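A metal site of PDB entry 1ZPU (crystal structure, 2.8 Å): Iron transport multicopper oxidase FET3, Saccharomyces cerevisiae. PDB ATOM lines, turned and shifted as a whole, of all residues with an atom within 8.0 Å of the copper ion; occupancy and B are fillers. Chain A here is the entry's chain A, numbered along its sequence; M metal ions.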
ATOM      1  N   GLU A 164     -17.602 -25.942 -32.510  1.00  0.00           N
ATOM      2  CA  GLU A 164     -17.461 -24.558 -32.090  1.00  0.00           C
ATOM      3  C   GLU A 164     -17.042 -23.690 -33.260  1.00  0.00           C
ATOM      4  O   GLU A 164     -16.173 -24.112 -34.032  1.00  0.00           O
ATOM      5  CB  GLU A 164     -16.372 -24.530 -31.025  1.00  0.00           C
ATOM      6  CG  GLU A 164     -15.421 -25.712 -31.220  1.00  0.00           C
ATOM      7  CD  GLU A 164     -15.264 -26.481 -29.951  1.00  0.00           C
ATOM      8  OE1 GLU A 164     -14.266 -27.232 -29.775  1.00  0.00           O
ATOM      9  OE2 GLU A 164     -16.165 -26.306 -29.107  1.00  0.00           O
ATOM     10  N   PHE A 198     -12.098 -18.710 -26.444  1.00  0.00           N
ATOM     11  CA  PHE A 198     -12.085 -20.061 -26.982  1.00  0.00           C
ATOM     12  C   PHE A 198     -10.692 -20.672 -26.935  1.00  0.00           C
ATOM     13  O   PHE A 198     -10.415 -21.531 -26.115  1.00  0.00           O
ATOM     14  CB  PHE A 198     -12.653 -20.033 -28.424  1.00  0.00           C
ATOM     15  CG  PHE A 198     -12.668 -21.362 -29.131  1.00  0.00           C
ATOM     16  CD1 PHE A 198     -12.636 -22.566 -28.436  1.00  0.00           C
ATOM     17  CD2 PHE A 198     -12.763 -21.401 -30.518  1.00  0.00           C
ATOM     18  CE1 PHE A 198     -12.673 -23.796 -29.116  1.00  0.00           C
ATOM     19  CE2 PHE A 198     -12.793 -22.643 -31.208  1.00  0.00           C
ATOM     20  CZ  PHE A 198     -12.752 -23.819 -30.501  1.00  0.00           C
ATOM     21  N   MET A 260      -7.893 -27.506 -31.166  1.00  0.00           N
ATOM     22  CA  MET A 260      -9.192 -27.176 -30.611  1.00  0.00           C
ATOM     23  C   MET A 260     -10.183 -26.782 -31.686  1.00  0.00           C
ATOM     24  O   MET A 260     -11.387 -26.733 -31.432  1.00  0.00           O
ATOM     25  CB  MET A 260      -9.034 -26.052 -29.568  1.00  0.00           C
ATOM     26  CG  MET A 260      -8.028 -26.429 -28.502  1.00  0.00           C
ATOM     27  SD  MET A 260      -7.720 -25.175 -27.268  1.00  0.00           S
ATOM     28  CE  MET A 260      -9.257 -25.136 -26.324  1.00  0.00           C
ATOM     29  N   VAL A 322     -16.997 -35.405 -18.202  1.00  0.00           N
ATOM     30  CA  VAL A 322     -17.285 -34.365 -19.180  1.00  0.00           C
ATOM     31  C   VAL A 322     -17.515 -34.982 -20.548  1.00  0.00           C
ATOM     32  O   VAL A 322     -16.635 -35.656 -21.087  1.00  0.00           O
ATOM     33  CB  VAL A 322     -16.114 -33.376 -19.279  1.00  0.00           C
ATOM     34  CG1 VAL A 322     -16.366 -32.379 -20.390  1.00  0.00           C
ATOM     35  CG2 VAL A 322     -15.899 -32.667 -17.955  1.00  0.00           C
ATOM     36  N   MET A 324     -19.880 -34.260 -24.507  1.00  0.00           N
ATOM     37  CA  MET A 324     -20.833 -33.559 -25.349  1.00  0.00           C
ATOM     38  C   MET A 324     -21.840 -34.585 -25.864  1.00  0.00           C
ATOM     39  O   MET A 324     -21.457 -35.695 -26.225  1.00  0.00           O
ATOM     40  CB  MET A 324     -20.106 -32.880 -26.523  1.00  0.00           C
ATOM     41  CG  MET A 324     -19.694 -31.420 -26.288  1.00  0.00           C
ATOM     42  SD  MET A 324     -18.779 -31.173 -24.756  1.00  0.00           S
ATOM     43  CE  MET A 324     -18.140 -29.513 -25.047  1.00  0.00           C
ATOM     44  N   ALA A 334     -23.354 -29.702 -23.509  1.00  0.00           N
ATOM     45  CA  ALA A 334     -22.222 -30.193 -22.721  1.00  0.00           C
ATOM     46  C   ALA A 334     -22.689 -30.652 -21.341  1.00  0.00           C
ATOM     47  O   ALA A 334     -23.577 -30.043 -20.746  1.00  0.00           O
ATOM     48  CB  ALA A 334     -21.209 -29.120 -22.584  1.00  0.00           C
ATOM     49  N   ASN A 386     -12.396 -36.315 -18.466  1.00  0.00           N
ATOM     50  CA  ASN A 386     -12.746 -35.929 -19.832  1.00  0.00           C
ATOM     51  C   ASN A 386     -13.078 -37.117 -20.710  1.00  0.00           C
ATOM     52  O   ASN A 386     -12.208 -37.941 -21.020  1.00  0.00           O
ATOM     53  CB  ASN A 386     -11.638 -35.102 -20.484  1.00  0.00           C
ATOM     54  CG  ASN A 386     -12.101 -34.406 -21.758  1.00  0.00           C
ATOM     55  OD1 ASN A 386     -13.297 -34.231 -21.976  1.00  0.00           O
ATOM     56  ND2 ASN A 386     -11.159 -34.007 -22.601  1.00  0.00           N
ATOM     57  N   ASP A 388     -14.515 -36.413 -23.587  1.00  0.00           N
ATOM     58  CA  ASP A 388     -14.488 -35.690 -24.859  1.00  0.00           C
ATOM     59  C   ASP A 388     -13.059 -35.630 -25.415  1.00  0.00           C
ATOM     60  O   ASP A 388     -12.099 -35.626 -24.633  1.00  0.00           O
ATOM     61  CB  ASP A 388     -15.018 -34.261 -24.666  1.00  0.00           C
ATOM     62  CG  ASP A 388     -14.921 -33.413 -25.928  1.00  0.00           C
ATOM     63  OD1 ASP A 388     -15.591 -33.753 -26.925  1.00  0.00           O
ATOM     64  OD2 ASP A 388     -14.172 -32.406 -25.936  1.00  0.00           O
ATOM     65  N   GLY A 390     -11.405 -33.256 -26.718  1.00  0.00           N
ATOM     66  CA  GLY A 390     -10.797 -31.921 -26.742  1.00  0.00           C
ATOM     67  C   GLY A 390     -10.123 -31.489 -25.447  1.00  0.00           C
ATOM     68  O   GLY A 390     -10.236 -32.167 -24.423  1.00  0.00           O
ATOM     69  N   THR A 391      -9.421 -30.360 -25.486  1.00  0.00           N
ATOM     70  CA  THR A 391      -8.849 -29.741 -24.299  1.00  0.00           C
ATOM     71  C   THR A 391      -9.838 -28.741 -23.736  1.00  0.00           C
ATOM     72  O   THR A 391     -10.442 -27.997 -24.485  1.00  0.00           O
ATOM     73  CB  THR A 391      -7.579 -28.954 -24.643  1.00  0.00           C
ATOM     74  OG1 THR A 391      -6.561 -29.867 -25.069  1.00  0.00           O
ATOM     75  CG2 THR A 391      -7.083 -28.209 -23.426  1.00  0.00           C
ATOM     76  N   HIS A 392      -9.987 -28.707 -22.410  1.00  0.00           N
ATOM     77  CA  HIS A 392     -10.855 -27.730 -21.768  1.00  0.00           C
ATOM     78  C   HIS A 392     -10.144 -27.100 -20.600  1.00  0.00           C
ATOM     79  O   HIS A 392      -9.567 -27.801 -19.748  1.00  0.00           O
ATOM     80  CB  HIS A 392     -12.119 -28.373 -21.254  1.00  0.00           C
ATOM     81  CG  HIS A 392     -12.812 -29.230 -22.258  1.00  0.00           C
ATOM     82  ND1 HIS A 392     -13.934 -28.814 -22.930  1.00  0.00           N
ATOM     83  CD2 HIS A 392     -12.558 -30.484 -22.689  1.00  0.00           C
ATOM     84  CE1 HIS A 392     -14.338 -29.764 -23.741  1.00  0.00           C
ATOM     85  NE2 HIS A 392     -13.521 -30.791 -23.614  1.00  0.00           N
ATOM     86  N   PRO A 393     -10.181 -25.761 -20.524  1.00  0.00           N
ATOM     87  CA  PRO A 393      -9.677 -25.089 -19.352  1.00  0.00           C
ATOM     88  C   PRO A 393     -10.820 -24.830 -18.342  1.00  0.00           C
ATOM     89  O   PRO A 393     -11.677 -23.992 -18.572  1.00  0.00           O
ATOM     90  CB  PRO A 393      -9.133 -23.789 -19.930  1.00  0.00           C
ATOM     91  CG  PRO A 393      -9.965 -23.547 -21.167  1.00  0.00           C
ATOM     92  CD  PRO A 393     -10.685 -24.810 -21.518  1.00  0.00           C
ATOM     93  N   PHE A 394     -10.824 -25.568 -17.252  1.00  0.00           N
ATOM     94  CA  PHE A 394     -11.830 -25.372 -16.235  1.00  0.00           C
ATOM     95  C   PHE A 394     -11.355 -24.376 -15.211  1.00  0.00           C
ATOM     96  O   PHE A 394     -10.177 -24.346 -14.848  1.00  0.00           O
ATOM     97  CB  PHE A 394     -12.232 -26.691 -15.578  1.00  0.00           C
ATOM     98  CG  PHE A 394     -12.997 -27.585 -16.485  1.00  0.00           C
ATOM     99  CD1 PHE A 394     -12.347 -28.550 -17.236  1.00  0.00           C
ATOM    100  CD2 PHE A 394     -14.370 -27.444 -16.636  1.00  0.00           C
ATOM    101  CE1 PHE A 394     -13.058 -29.369 -18.107  1.00  0.00           C
ATOM    102  CE2 PHE A 394     -15.083 -28.273 -17.508  1.00  0.00           C
ATOM    103  CZ  PHE A 394     -14.411 -29.235 -18.239  1.00  0.00           C
ATOM    104  N   VAL A 441      -7.772 -29.869 -18.683  1.00  0.00           N
ATOM    105  CA  VAL A 441      -7.654 -31.305 -18.917  1.00  0.00           C
ATOM    106  C   VAL A 441      -7.187 -31.526 -20.336  1.00  0.00           C
ATOM    107  O   VAL A 441      -7.641 -30.826 -21.258  1.00  0.00           O
ATOM    108  CB  VAL A 441      -8.977 -32.074 -18.882  1.00  0.00           C
ATOM    109  CG1 VAL A 441      -8.961 -33.152 -17.817  1.00  0.00           C
ATOM    110  CG2 VAL A 441     -10.175 -31.142 -18.815  1.00  0.00           C
ATOM    111  N   HIS A 462     -16.709 -24.279 -13.993  1.00  0.00           N
ATOM    112  CA  HIS A 462     -17.062 -24.478 -15.391  1.00  0.00           C
ATOM    113  C   HIS A 462     -15.876 -24.400 -16.317  1.00  0.00           C
ATOM    114  O   HIS A 462     -14.800 -23.919 -15.951  1.00  0.00           O
ATOM    115  CB  HIS A 462     -18.063 -23.414 -15.826  1.00  0.00           C
ATOM    116  CG  HIS A 462     -17.500 -22.025 -15.816  1.00  0.00           C
ATOM    117  ND1 HIS A 462     -16.891 -21.462 -16.918  1.00  0.00           N
ATOM    118  CD2 HIS A 462     -17.435 -21.098 -14.837  1.00  0.00           C
ATOM    119  CE1 HIS A 462     -16.479 -20.247 -16.620  1.00  0.00           C
ATOM    120  NE2 HIS A 462     -16.785 -20.002 -15.359  1.00  0.00           N
ATOM    121  N   CYS A 463     -16.107 -24.827 -17.551  1.00  0.00           N
ATOM    122  CA  CYS A 463     -15.183 -24.604 -18.638  1.00  0.00           C
ATOM    123  C   CYS A 463     -15.245 -23.137 -19.073  1.00  0.00           C
ATOM    124  O   CYS A 463     -16.317 -22.563 -19.243  1.00  0.00           O
ATOM    125  CB  CYS A 463     -15.521 -25.517 -19.806  1.00  0.00           C
ATOM    126  SG  CYS A 463     -14.357 -25.381 -21.149  1.00  0.00           S
ATOM    127  N   HIS A 464     -14.081 -22.539 -19.261  1.00  0.00           N
ATOM    128  CA  HIS A 464     -13.995 -21.145 -19.611  1.00  0.00           C
ATOM    129  C   HIS A 464     -14.052 -20.882 -21.127  1.00  0.00           C
ATOM    130  O   HIS A 464     -13.913 -19.750 -21.566  1.00  0.00           O
ATOM    131  CB  HIS A 464     -12.762 -20.510 -19.004  1.00  0.00           C
ATOM    132  CG  HIS A 464     -12.965 -19.092 -18.591  1.00  0.00           C
ATOM    133  ND1 HIS A 464     -13.079 -18.068 -19.510  1.00  0.00           N
ATOM    134  CD2 HIS A 464     -13.098 -18.521 -17.367  1.00  0.00           C
ATOM    135  CE1 HIS A 464     -13.280 -16.930 -18.867  1.00  0.00           C
ATOM    136  NE2 HIS A 464     -13.286 -17.179 -17.561  1.00  0.00           N
ATOM    137  N   ILE A 465     -14.267 -21.934 -21.914  1.00  0.00           N
ATOM    138  CA  ILE A 465     -14.493 -21.752 -23.325  1.00  0.00           C
ATOM    139  C   ILE A 465     -15.941 -21.348 -23.457  1.00  0.00           C
ATOM    140  O   ILE A 465     -16.841 -22.119 -23.161  1.00  0.00           O
ATOM    141  CB  ILE A 465     -14.259 -23.046 -24.130  1.00  0.00           C
ATOM    142  CG1 ILE A 465     -12.750 -23.336 -24.250  1.00  0.00           C
ATOM    143  CG2 ILE A 465     -14.923 -22.929 -25.525  1.00  0.00           C
ATOM    144  CD1 ILE A 465     -12.436 -24.728 -24.761  1.00  0.00           C
ATOM    145  N   GLU A 466     -16.148 -20.117 -23.920  1.00  0.00           N
ATOM    146  CA  GLU A 466     -17.459 -19.512 -23.937  1.00  0.00           C
ATOM    147  C   GLU A 466     -18.533 -20.370 -24.600  1.00  0.00           C
ATOM    148  O   GLU A 466     -19.674 -20.440 -24.124  1.00  0.00           O
ATOM    149  CB  GLU A 466     -17.356 -18.144 -24.580  1.00  0.00           C
ATOM    150  CG  GLU A 466     -16.924 -17.081 -23.571  1.00  0.00           C
ATOM    151  CD  GLU A 466     -18.067 -16.681 -22.620  1.00  0.00           C
ATOM    152  OE1 GLU A 466     -19.042 -16.040 -23.116  1.00  0.00           O
ATOM    153  OE2 GLU A 466     -17.989 -17.023 -21.412  1.00  0.00           O
ATOM    154  N   TRP A 467     -18.155 -21.038 -25.691  1.00  0.00           N
ATOM    155  CA  TRP A 467     -19.069 -21.922 -26.396  1.00  0.00           C
ATOM    156  C   TRP A 467     -19.513 -23.086 -25.518  1.00  0.00           C
ATOM    157  O   TRP A 467     -20.677 -23.470 -25.536  1.00  0.00           O
ATOM    158  CB  TRP A 467     -18.413 -22.420 -27.675  1.00  0.00           C
ATOM    159  CG  TRP A 467     -17.789 -21.316 -28.498  1.00  0.00           C
ATOM    160  CD1 TRP A 467     -16.469 -21.157 -28.787  1.00  0.00           C
ATOM    161  CD2 TRP A 467     -18.477 -20.210 -29.110  1.00  0.00           C
ATOM    162  NE1 TRP A 467     -16.285 -20.025 -29.568  1.00  0.00           N
ATOM    163  CE2 TRP A 467     -17.507 -19.423 -29.765  1.00  0.00           C
ATOM    164  CE3 TRP A 467     -19.821 -19.811 -29.172  1.00  0.00           C
ATOM    165  CZ2 TRP A 467     -17.826 -18.267 -30.474  1.00  0.00           C
ATOM    166  CZ3 TRP A 467     -20.140 -18.655 -29.871  1.00  0.00           C
ATOM    167  CH2 TRP A 467     -19.147 -17.897 -30.518  1.00  0.00           C
ATOM    168  N   HIS A 468     -18.588 -23.638 -24.735  1.00  0.00           N
ATOM    169  CA  HIS A 468     -18.898 -24.777 -23.905  1.00  0.00           C
ATOM    170  C   HIS A 468     -19.748 -24.392 -22.684  1.00  0.00           C
ATOM    171  O   HIS A 468     -20.595 -25.171 -22.219  1.00  0.00           O
ATOM    172  CB  HIS A 468     -17.623 -25.524 -23.517  1.00  0.00           C
ATOM    173  CG  HIS A 468     -16.847 -26.046 -24.687  1.00  0.00           C
ATOM    174  ND1 HIS A 468     -15.561 -26.536 -24.572  1.00  0.00           N
ATOM    175  CD2 HIS A 468     -17.165 -26.137 -25.997  1.00  0.00           C
ATOM    176  CE1 HIS A 468     -15.129 -26.919 -25.762  1.00  0.00           C
ATOM    177  NE2 HIS A 468     -16.079 -26.677 -26.647  1.00  0.00           N
ATOM    178  N   LEU A 469     -19.511 -23.181 -22.166  1.00  0.00           N
ATOM    179  CA  LEU A 469     -20.338 -22.645 -21.105  1.00  0.00           C
ATOM    180  C   LEU A 469     -21.763 -22.409 -21.620  1.00  0.00           C
ATOM    181  O   LEU A 469     -22.733 -22.655 -20.896  1.00  0.00           O
ATOM    182  CB  LEU A 469     -19.733 -21.359 -20.581  1.00  0.00           C
ATOM    183  CG  LEU A 469     -20.396 -20.674 -19.389  1.00  0.00           C
ATOM    184  CD1 LEU A 469     -20.435 -21.571 -18.130  1.00  0.00           C
ATOM    185  CD2 LEU A 469     -19.696 -19.335 -19.132  1.00  0.00           C
ATOM    186  N   GLN A 471     -23.061 -24.226 -23.897  1.00  0.00           N
ATOM    187  CA  GLN A 471     -23.548 -25.602 -23.966  1.00  0.00           C
ATOM    188  C   GLN A 471     -23.889 -26.162 -22.592  1.00  0.00           C
ATOM    189  O   GLN A 471     -24.351 -27.297 -22.484  1.00  0.00           O
ATOM    190  CB  GLN A 471     -22.509 -26.461 -24.659  1.00  0.00           C
ATOM    191  CG  GLN A 471     -22.437 -26.291 -26.160  1.00  0.00           C
ATOM    192  CD  GLN A 471     -21.421 -27.233 -26.759  1.00  0.00           C
ATOM    193  OE1 GLN A 471     -20.236 -26.910 -26.856  1.00  0.00           O
ATOM    194  NE2 GLN A 471     -21.871 -28.428 -27.166  1.00  0.00           N
ATOM    195  N   LEU A 473     -21.621 -26.413 -19.662  1.00  0.00           N
ATOM    196  CA  LEU A 473     -20.568 -27.156 -18.963  1.00  0.00           C
ATOM    197  C   LEU A 473     -20.217 -26.444 -17.679  1.00  0.00           C
ATOM    198  O   LEU A 473     -19.149 -25.837 -17.575  1.00  0.00           O
ATOM    199  CB  LEU A 473     -19.309 -27.252 -19.822  1.00  0.00           C
ATOM    200  CG  LEU A 473     -18.635 -28.625 -19.961  1.00  0.00           C
ATOM    201  CD1 LEU A 473     -17.194 -28.501 -20.432  1.00  0.00           C
ATOM    202  CD2 LEU A 473     -18.709 -29.500 -18.710  1.00  0.00           C
HETATM  203 CU    CU M   1     -14.618 -26.864 -22.750  1.00  0.00          CU
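A ring nitrogen (NE2) of His 392 sits at hydrogen-bond distance from the side-chain carboxylate (OD2) of Asp 388 (2.9 Å). The backbone NH of Val 441 is in hydrogen-bond range of the backbone carbonyl oxygen of His 392. The backbone NH of Leu 473 is in hydrogen-bond range of the backbone carbonyl oxygen of His 468 (3.0 Å). A ring nitrogen (NE2) of His 468 is in hydrogen-bond range of the side-chain carboxylate (OE2) of Glu 164. The side-chain sulfur (SG) of Cys 463 sits close to the backbone NH (N) of Ile 465, 3.5 Å away. The backbone carbonyl oxygen (O) of Leu 473 lies within hydrogen-bond range of the backbone NH (N) of Cys 463 (3.2 Å).
Merely in contact with the copper ion: Ile 465 (3.7 Å) and Leu 473 (3.8 Å). Of the 24 residues printed, 5 come within 4 Å of the copper ion.
The copper ion is bound by a ring nitrogen (ND1) of His 392 (2.1 Å), a ring nitrogen (ND1) of His 468 (2.1 Å) and the side-chain sulfur of Cys 463 (2.2 Å). The copper ion has three donor atoms within binding distance.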
